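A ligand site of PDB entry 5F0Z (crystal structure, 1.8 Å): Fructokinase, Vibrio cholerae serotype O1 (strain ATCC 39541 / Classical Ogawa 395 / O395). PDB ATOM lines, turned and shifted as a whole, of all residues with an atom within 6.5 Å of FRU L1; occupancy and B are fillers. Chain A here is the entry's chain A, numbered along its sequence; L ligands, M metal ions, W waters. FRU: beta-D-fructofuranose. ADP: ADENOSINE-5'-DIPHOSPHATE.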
ATOM      1  N   ASP A  26      -0.799 -39.314  16.419  1.00  0.00           N
ATOM      2  CA  ASP A  26      -2.239 -39.036  16.362  1.00  0.00           C
ATOM      3  C   ASP A  26      -2.658 -38.252  15.130  1.00  0.00           C
ATOM      4  O   ASP A  26      -2.203 -37.119  14.929  1.00  0.00           O
ATOM      5  CB  ASP A  26      -2.701 -38.298  17.616  1.00  0.00           C
ATOM      6  CG  ASP A  26      -2.026 -36.939  17.808  1.00  0.00           C
ATOM      7  OD1 ASP A  26      -2.736 -35.971  18.160  1.00  0.00           O
ATOM      8  OD2 ASP A  26      -0.781 -36.824  17.681  1.00  0.00           O
ATOM      9  N   ALA A  27      -3.497 -38.889  14.326  1.00  0.00           N
ATOM     10  CA  ALA A  27      -4.304 -38.213  13.319  1.00  0.00           C
ATOM     11  C   ALA A  27      -5.629 -37.868  13.988  1.00  0.00           C
ATOM     12  O   ALA A  27      -6.231 -38.679  14.677  1.00  0.00           O
ATOM     13  CB  ALA A  27      -4.521 -39.116  12.118  1.00  0.00           C
ATOM     14  N   VAL A  28      -6.077 -36.643  13.768  1.00  0.00           N
ATOM     15  CA  VAL A  28      -7.140 -36.052  14.562  1.00  0.00           C
ATOM     16  C   VAL A  28      -8.048 -35.249  13.640  1.00  0.00           C
ATOM     17  O   VAL A  28      -7.587 -34.663  12.659  1.00  0.00           O
ATOM     18  CB  VAL A  28      -6.478 -35.029  15.511  1.00  0.00           C
ATOM     19  CG1 VAL A  28      -7.443 -34.113  16.146  1.00  0.00           C
ATOM     20  CG2 VAL A  28      -5.552 -35.763  16.512  1.00  0.00           C
ATOM     21  N   VAL A  29      -9.331 -35.205  13.963  1.00  0.00           N
ATOM     22  CA  VAL A  29     -10.211 -34.190  13.399  1.00  0.00           C
ATOM     23  C   VAL A  29     -10.259 -32.979  14.328  1.00  0.00           C
ATOM     24  O   VAL A  29     -10.636 -33.073  15.496  1.00  0.00           O
ATOM     25  CB  VAL A  29     -11.631 -34.732  13.130  1.00  0.00           C
ATOM     26  CG1 VAL A  29     -12.574 -33.607  12.753  1.00  0.00           C
ATOM     27  CG2 VAL A  29     -11.584 -35.757  12.033  1.00  0.00           C
ATOM     28  N   ASP A  30      -9.869 -31.831  13.766  1.00  0.00           N
ATOM     29  CA  ASP A  30      -9.892 -30.577  14.488  1.00  0.00           C
ATOM     30  C   ASP A  30     -11.175 -29.884  14.083  1.00  0.00           C
ATOM     31  O   ASP A  30     -11.409 -29.648  12.880  1.00  0.00           O
ATOM     32  CB  ASP A  30      -8.716 -29.666  14.087  1.00  0.00           C
ATOM     33  CG  ASP A  30      -7.360 -30.079  14.704  1.00  0.00           C
ATOM     34  OD1 ASP A  30      -7.304 -30.676  15.777  1.00  0.00           O
ATOM     35  OD2 ASP A  30      -6.339 -29.738  14.081  1.00  0.00           O
ATOM     36  N   PRO A  43      -8.948 -31.797   8.880  1.00  0.00           N
ATOM     37  CA  PRO A  43      -7.984 -32.848   9.189  1.00  0.00           C
ATOM     38  C   PRO A  43      -6.817 -32.239   9.954  1.00  0.00           C
ATOM     39  O   PRO A  43      -6.371 -31.113   9.690  1.00  0.00           O
ATOM     40  CB  PRO A  43      -7.581 -33.348   7.801  1.00  0.00           C
ATOM     41  CG  PRO A  43      -7.749 -32.164   6.903  1.00  0.00           C
ATOM     42  CD  PRO A  43      -8.984 -31.483   7.444  1.00  0.00           C
ATOM     43  N   GLY A  44      -6.286 -32.999  10.906  1.00  0.00           N
ATOM     44  CA  GLY A  44      -5.225 -32.517  11.751  1.00  0.00           C
ATOM     45  C   GLY A  44      -4.496 -33.634  12.487  1.00  0.00           C
ATOM     46  O   GLY A  44      -4.549 -34.771  12.070  1.00  0.00           O
ATOM     47  N   GLY A  45      -3.846 -33.299  13.588  1.00  0.00           N
ATOM     48  CA  GLY A  45      -2.998 -34.222  14.306  1.00  0.00           C
ATOM     49  C   GLY A  45      -1.569 -33.948  13.886  1.00  0.00           C
ATOM     50  O   GLY A  45      -1.255 -34.110  12.722  1.00  0.00           O
ATOM     51  N   ALA A  46      -0.727 -33.514  14.824  1.00  0.00           N
ATOM     52  CA  ALA A  46       0.601 -33.003  14.499  1.00  0.00           C
ATOM     53  C   ALA A  46       1.416 -33.902  13.570  1.00  0.00           C
ATOM     54  O   ALA A  46       1.896 -33.455  12.527  1.00  0.00           O
ATOM     55  CB  ALA A  46       1.383 -32.707  15.786  1.00  0.00           C
ATOM     56  N   PRO A  47       1.519 -35.196  13.900  1.00  0.00           N
ATOM     57  CA  PRO A  47       2.330 -35.988  12.964  1.00  0.00           C
ATOM     58  C   PRO A  47       1.649 -36.180  11.620  1.00  0.00           C
ATOM     59  O   PRO A  47       2.341 -36.313  10.605  1.00  0.00           O
ATOM     60  CB  PRO A  47       2.510 -37.325  13.683  1.00  0.00           C
ATOM     61  CG  PRO A  47       1.498 -37.378  14.720  1.00  0.00           C
ATOM     62  CD  PRO A  47       1.157 -35.980  15.099  1.00  0.00           C
ATOM     63  N   ASN A  49      -0.111 -33.815  10.252  1.00  0.00           N
ATOM     64  CA  ASN A  49       0.195 -32.533   9.624  1.00  0.00           C
ATOM     65  C   ASN A  49       1.588 -32.535   9.024  1.00  0.00           C
ATOM     66  O   ASN A  49       1.786 -32.112   7.885  1.00  0.00           O
ATOM     67  CB  ASN A  49       0.083 -31.395  10.656  1.00  0.00           C
ATOM     68  CG  ASN A  49      -1.315 -31.239  11.222  1.00  0.00           C
ATOM     69  OD1 ASN A  49      -2.303 -31.644  10.604  1.00  0.00           O
ATOM     70  ND2 ASN A  49      -1.421 -30.653  12.417  1.00  0.00           N
ATOM     71  N   SER A  99      -9.275 -39.451  17.624  1.00  0.00           N
ATOM     72  CA  SER A  99      -9.142 -38.224  18.385  1.00  0.00           C
ATOM     73  C   SER A  99      -9.933 -37.114  17.714  1.00  0.00           C
ATOM     74  O   SER A  99      -9.889 -36.939  16.492  1.00  0.00           O
ATOM     75  CB  SER A  99      -7.686 -37.824  18.461  1.00  0.00           C
ATOM     76  OG  SER A  99      -7.562 -36.670  19.226  1.00  0.00           O
ATOM     77  N   VAL A 101     -10.785 -33.002  18.421  1.00  0.00           N
ATOM     78  CA  VAL A 101     -10.273 -31.835  19.149  1.00  0.00           C
ATOM     79  C   VAL A 101     -11.058 -30.595  18.790  1.00  0.00           C
ATOM     80  O   VAL A 101     -11.325 -30.359  17.632  1.00  0.00           O
ATOM     81  CB  VAL A 101      -8.782 -31.592  18.804  1.00  0.00           C
ATOM     82  CG1 VAL A 101      -8.282 -30.285  19.382  1.00  0.00           C
ATOM     83  CG2 VAL A 101      -7.922 -32.743  19.297  1.00  0.00           C
ATOM     84  N   VAL A 103     -11.177 -26.530  18.764  1.00  0.00           N
ATOM     85  CA  VAL A 103     -10.225 -25.425  18.737  1.00  0.00           C
ATOM     86  C   VAL A 103     -10.918 -24.130  19.150  1.00  0.00           C
ATOM     87  O   VAL A 103     -12.046 -23.842  18.724  1.00  0.00           O
ATOM     88  CB  VAL A 103      -9.591 -25.259  17.335  1.00  0.00           C
ATOM     89  CG1 VAL A 103      -8.613 -24.086  17.308  1.00  0.00           C
ATOM     90  CG2 VAL A 103      -8.927 -26.532  16.884  1.00  0.00           C
ATOM     91  N   GLY A 109      -1.853 -22.369  20.271  1.00  0.00           N
ATOM     92  CA  GLY A 109      -1.088 -23.515  20.720  1.00  0.00           C
ATOM     93  C   GLY A 109      -1.886 -24.384  21.661  1.00  0.00           C
ATOM     94  O   GLY A 109      -3.118 -24.502  21.537  1.00  0.00           O
ATOM     95  N   PHE A 113      -6.649 -25.958  22.395  1.00  0.00           N
ATOM     96  CA  PHE A 113      -7.211 -27.284  22.096  1.00  0.00           C
ATOM     97  C   PHE A 113      -7.921 -27.907  23.283  1.00  0.00           C
ATOM     98  O   PHE A 113      -7.418 -27.843  24.393  1.00  0.00           O
ATOM     99  CB  PHE A 113      -6.094 -28.242  21.637  1.00  0.00           C
ATOM    100  CG  PHE A 113      -5.343 -27.750  20.416  1.00  0.00           C
ATOM    101  CD1 PHE A 113      -4.009 -27.369  20.525  1.00  0.00           C
ATOM    102  CD2 PHE A 113      -5.967 -27.627  19.191  1.00  0.00           C
ATOM    103  CE1 PHE A 113      -3.317 -26.901  19.426  1.00  0.00           C
ATOM    104  CE2 PHE A 113      -5.281 -27.145  18.079  1.00  0.00           C
ATOM    105  CZ  PHE A 113      -3.964 -26.780  18.195  1.00  0.00           C
ATOM    106  N   PHE A 115      -9.327 -31.759  24.035  1.00  0.00           N
ATOM    107  CA  PHE A 115      -9.329 -33.119  23.515  1.00  0.00           C
ATOM    108  C   PHE A 115     -10.556 -33.881  24.033  1.00  0.00           C
ATOM    109  O   PHE A 115     -10.654 -34.166  25.211  1.00  0.00           O
ATOM    110  CB  PHE A 115      -8.042 -33.836  23.923  1.00  0.00           C
ATOM    111  CG  PHE A 115      -6.838 -33.332  23.194  1.00  0.00           C
ATOM    112  CD1 PHE A 115      -6.347 -34.020  22.099  1.00  0.00           C
ATOM    113  CD2 PHE A 115      -6.236 -32.129  23.543  1.00  0.00           C
ATOM    114  CE1 PHE A 115      -5.252 -33.533  21.400  1.00  0.00           C
ATOM    115  CE2 PHE A 115      -5.139 -31.649  22.820  1.00  0.00           C
ATOM    116  CZ  PHE A 115      -4.661 -32.350  21.749  1.00  0.00           C
ATOM    117  N   ILE A 144       2.308 -36.525  22.369  1.00  0.00           N
ATOM    118  CA  ILE A 144       1.058 -37.218  22.577  1.00  0.00           C
ATOM    119  C   ILE A 144       1.257 -38.739  22.449  1.00  0.00           C
ATOM    120  O   ILE A 144       0.645 -39.532  23.192  1.00  0.00           O
ATOM    121  CB  ILE A 144      -0.070 -36.674  21.649  1.00  0.00           C
ATOM    122  CG1 ILE A 144      -0.733 -35.449  22.291  1.00  0.00           C
ATOM    123  CG2 ILE A 144      -1.145 -37.740  21.439  1.00  0.00           C
ATOM    124  CD1 ILE A 144      -1.841 -34.833  21.399  1.00  0.00           C
ATOM    125  N   ASN A 174       5.573 -30.701  21.366  1.00  0.00           N
ATOM    126  CA  ASN A 174       4.209 -30.393  21.007  1.00  0.00           C
ATOM    127  C   ASN A 174       3.275 -30.732  22.164  1.00  0.00           C
ATOM    128  O   ASN A 174       2.346 -31.566  22.055  1.00  0.00           O
ATOM    129  CB  ASN A 174       3.831 -31.171  19.749  1.00  0.00           C
ATOM    130  CG  ASN A 174       3.294 -30.286  18.659  1.00  0.00           C
ATOM    131  OD1 ASN A 174       2.865 -29.172  18.903  1.00  0.00           O
ATOM    132  ND2 ASN A 174       3.308 -30.791  17.422  1.00  0.00           N
ATOM    133  N   ARG A 176       0.639 -31.316  24.976  1.00  0.00           N
ATOM    134  CA  ARG A 176      -0.799 -31.226  25.220  1.00  0.00           C
ATOM    135  C   ARG A 176      -1.074 -31.993  26.503  1.00  0.00           C
ATOM    136  O   ARG A 176      -1.424 -33.164  26.498  1.00  0.00           O
ATOM    137  CB  ARG A 176      -1.587 -31.852  24.045  1.00  0.00           C
ATOM    138  CG  ARG A 176      -1.179 -31.331  22.673  1.00  0.00           C
ATOM    139  CD  ARG A 176      -1.666 -29.880  22.389  1.00  0.00           C
ATOM    140  NE  ARG A 176      -1.372 -29.557  20.998  1.00  0.00           N
ATOM    141  CZ  ARG A 176      -0.243 -29.017  20.534  1.00  0.00           C
ATOM    142  NH1 ARG A 176       0.717 -28.621  21.366  1.00  0.00           N
ATOM    143  NH2 ARG A 176      -0.079 -28.833  19.238  1.00  0.00           N
ATOM    144  N   THR A 262      -3.137 -22.642  13.988  1.00  0.00           N
ATOM    145  CA  THR A 262      -3.219 -24.082  14.234  1.00  0.00           C
ATOM    146  C   THR A 262      -2.268 -24.849  13.338  1.00  0.00           C
ATOM    147  O   THR A 262      -2.363 -24.772  12.119  1.00  0.00           O
ATOM    148  CB  THR A 262      -4.654 -24.609  13.972  1.00  0.00           C
ATOM    149  OG1 THR A 262      -5.592 -23.904  14.799  1.00  0.00           O
ATOM    150  CG2 THR A 262      -4.764 -26.109  14.243  1.00  0.00           C
ATOM    151  N   GLY A 263      -1.361 -25.601  13.936  1.00  0.00           N
ATOM    152  CA  GLY A 263      -0.459 -26.429  13.148  1.00  0.00           C
ATOM    153  C   GLY A 263       0.694 -25.709  12.469  1.00  0.00           C
ATOM    154  O   GLY A 263       1.427 -26.329  11.700  1.00  0.00           O
ATOM    155  N   ALA A 264       0.863 -24.417  12.695  1.00  0.00           N
ATOM    156  CA  ALA A 264       1.983 -23.697  12.060  1.00  0.00           C
ATOM    157  C   ALA A 264       3.344 -24.323  12.439  1.00  0.00           C
ATOM    158  O   ALA A 264       4.265 -24.388  11.621  1.00  0.00           O
ATOM    159  CB  ALA A 264       1.944 -22.212  12.397  1.00  0.00           C
ATOM    160  N   GLY A 265       3.484 -24.779  13.682  1.00  0.00           N
ATOM    161  CA  GLY A 265       4.728 -25.384  14.134  1.00  0.00           C
ATOM    162  C   GLY A 265       4.993 -26.722  13.460  1.00  0.00           C
ATOM    163  O   GLY A 265       6.155 -27.119  13.275  1.00  0.00           O
ATOM    164  N   ASP A 266       3.921 -27.412  13.050  1.00  0.00           N
ATOM    165  CA  ASP A 266       4.054 -28.666  12.295  1.00  0.00           C
ATOM    166  C   ASP A 266       4.439 -28.422  10.842  1.00  0.00           C
ATOM    167  O   ASP A 266       5.200 -29.197  10.248  1.00  0.00           O
ATOM    168  CB  ASP A 266       2.752 -29.483  12.322  1.00  0.00           C
ATOM    169  CG  ASP A 266       2.270 -29.779  13.717  1.00  0.00           C
ATOM    170  OD1 ASP A 266       3.112 -29.954  14.627  1.00  0.00           O
ATOM    171  OD2 ASP A 266       1.013 -29.859  13.901  1.00  0.00           O
ATOM    172  N   ALA A 308      -4.984 -26.953  10.093  1.00  0.00           N
ATOM    173  CA  ALA A 308      -3.548 -27.178  10.087  1.00  0.00           C
ATOM    174  C   ALA A 308      -2.976 -27.508   8.711  1.00  0.00           C
ATOM    175  O   ALA A 308      -1.856 -27.107   8.378  1.00  0.00           O
ATOM    176  CB  ALA A 308      -3.187 -28.274  11.066  1.00  0.00           C
HETATM  177  C1  FRU L   1      -2.685 -32.599  18.484  1.00  0.00           C
HETATM  178  C2  FRU L   1      -2.964 -31.246  17.901  1.00  0.00           C
HETATM  179  C3  FRU L   1      -4.009 -31.249  16.852  1.00  0.00           C
HETATM  180  C4  FRU L   1      -3.529 -30.185  15.921  1.00  0.00           C
HETATM  181  C5  FRU L   1      -2.040 -30.239  16.099  1.00  0.00           C
HETATM  182  C6  FRU L   1      -1.329 -28.928  15.880  1.00  0.00           C
HETATM  183  O1  FRU L   1      -2.108 -33.468  17.571  1.00  0.00           O
HETATM  184  O2  FRU L   1      -3.351 -30.423  18.939  1.00  0.00           O
HETATM  185  O3  FRU L   1      -5.277 -30.946  17.406  1.00  0.00           O
HETATM  186  O4  FRU L   1      -3.837 -30.452  14.590  1.00  0.00           O
HETATM  187  O5  FRU L   1      -1.796 -30.673  17.409  1.00  0.00           O
HETATM  188  O6  FRU L   1       0.054 -29.089  16.038  1.00  0.00           O
HETATM  189  PB  ADP L   2       1.886 -23.653  16.077  1.00  0.00           P
HETATM  190  O1B ADP L   2       0.606 -24.307  15.602  1.00  0.00           O
HETATM  191  O2B ADP L   2       1.629 -23.143  17.487  1.00  0.00           O
HETATM  192  O3B ADP L   2       2.956 -24.723  16.140  1.00  0.00           O
HETATM  193  PA  ADP L   2       3.085 -21.147  15.814  1.00  0.00           P
HETATM  194  O1A ADP L   2       2.058 -20.063  15.943  1.00  0.00           O
HETATM  195  O2A ADP L   2       3.685 -21.383  17.187  1.00  0.00           O
HETATM  196  O3A ADP L   2       2.356 -22.424  15.232  1.00  0.00           O
HETATM  197  O5' ADP L   2       4.271 -20.754  14.796  1.00  0.00           O
HETATM  198  C5' ADP L   2       5.627 -21.095  14.916  1.00  0.00           C
HETATM  199  C4' ADP L   2       6.450 -21.068  13.633  1.00  0.00           C
HETATM  200  O4' ADP L   2       5.693 -20.809  12.488  1.00  0.00           O
HETATM  201  C3' ADP L   2       7.558 -20.046  13.693  1.00  0.00           C
HETATM  202  O3' ADP L   2       8.803 -20.600  13.881  1.00  0.00           O
HETATM  203  C2' ADP L   2       7.537 -19.388  12.382  1.00  0.00           C
HETATM  204  O2' ADP L   2       8.457 -19.904  11.488  1.00  0.00           O
HETATM  205  C1' ADP L   2       6.160 -19.614  11.910  1.00  0.00           C
HETATM  206  N9  ADP L   2       5.383 -18.462  12.285  1.00  0.00           N
HETATM  207  C8  ADP L   2       4.538 -18.366  13.314  1.00  0.00           C
HETATM  208  N7  ADP L   2       3.998 -17.167  13.393  1.00  0.00           N
HETATM  209  C5  ADP L   2       4.482 -16.422  12.401  1.00  0.00           C
HETATM  210  C6  ADP L   2       4.274 -15.113  11.997  1.00  0.00           C
HETATM  211  N6  ADP L   2       3.368 -14.278  12.718  1.00  0.00           N
HETATM  212  N1  ADP L   2       4.931 -14.638  10.936  1.00  0.00           N
HETATM  213  C2  ADP L   2       5.786 -15.415  10.252  1.00  0.00           C
HETATM  214  N3  ADP L   2       6.010 -16.692  10.622  1.00  0.00           N
HETATM  215  C4  ADP L   2       5.378 -17.229  11.683  1.00  0.00           C
HETATM  216 CA    CA M   1       3.598 -27.124  18.248  1.00  0.00          CA
HETATM  217  O   HOH W   1       1.588 -26.854  17.002  1.00  0.00           O
HETATM  218  O   HOH W   2       0.464 -34.424  18.551  1.00  0.00           O
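An oxygen (O4) of FRU L1 sits at hydrogen-bond distance from the backbone NH of Gly 45, at 3.0 Å.
N of Ala 46 sits at hydrogen-bond distance from O1 of FRU L1, 3.1 Å away.
OD2 of Asp 266 lies within hydrogen-bond range of O6 of FRU L1, 2.5 Å away.
N of Gly 263 is in hydrogen-bond range of O1B of ADP L2 (2.9 Å).
NE of Arg 176 is in hydrogen-bond range of O2 of FRU L1.
The backbone NH (N) of Ala 264 is in hydrogen-bond range of an oxygen (O1B) of ADP L2 (2.9 Å).
The side-chain amide nitrogen (ND2) of Asn 49 sits at hydrogen-bond distance from an oxygen (O4) of FRU L1.
The side-chain carboxylate (OD1) of Asp 30 is in hydrogen-bond range of an oxygen (O3) of FRU L1 (2.6 Å).
The backbone NH of Gly 265 is in hydrogen-bond range of an oxygen (O3B) of ADP L2 (2.5 Å).
The side-chain carboxylate (OD1) of Asp 26 sits at hydrogen-bond distance from an oxygen (O1) of FRU L1, at 2.6 Å.
OD2 of Asp 266 lies within hydrogen-bond range of ND2 of Asn 49.
The side-chain amide oxygen of Asn 49 lies close to the backbone carbonyl oxygen of Gly 45 (3.4 Å).
The guanidinium group of Arg 176 lies close to the backbone carbonyl oxygen of Asn 174 (3.4 Å).
The side-chain carboxylate (OD1) of Asp 266 is in hydrogen-bond range of the side-chain amide nitrogen (ND2) of Asn 174, 2.9 Å away.
N of Gly 44 is in hydrogen-bond range of O of Val 28 (2.7 Å).
N of Val 101 sits at hydrogen-bond distance from O of Val 29 (2.9 Å).
Merely in contact with FRU L1: Gly 44, Val 101, Phe 113, Phe 115, Ile 144, Asn 174 and Gly 263.
Hydrophobic or aromatic side chains that line FRU L1: Ala 46, Val 101, Phe 113, Phe 115 and Ile 144.
14 residues have an atom within 4 Å of FRU L1: Asp 26, Asp 30, Gly 44, Gly 45, Ala 46, Asn 49, Val 101, Phe 113, Phe 115, Ile 144, Asn 174, Arg 176, Gly 263 and Asp 266.
The nearest printed residue that does not touch FRU L1 is Val 28 (4.04 Å).
Water W1 lies within hydrogen-bond range of O3B of ADP L2 (2.7 Å), O6 of FRU L1 (2.9 Å) and NH2 of Arg 176 (3.4 Å).
Water W2 bridges the side-chain carboxylate (OD2) of Asp 26 and an oxygen (O1) of FRU L1.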
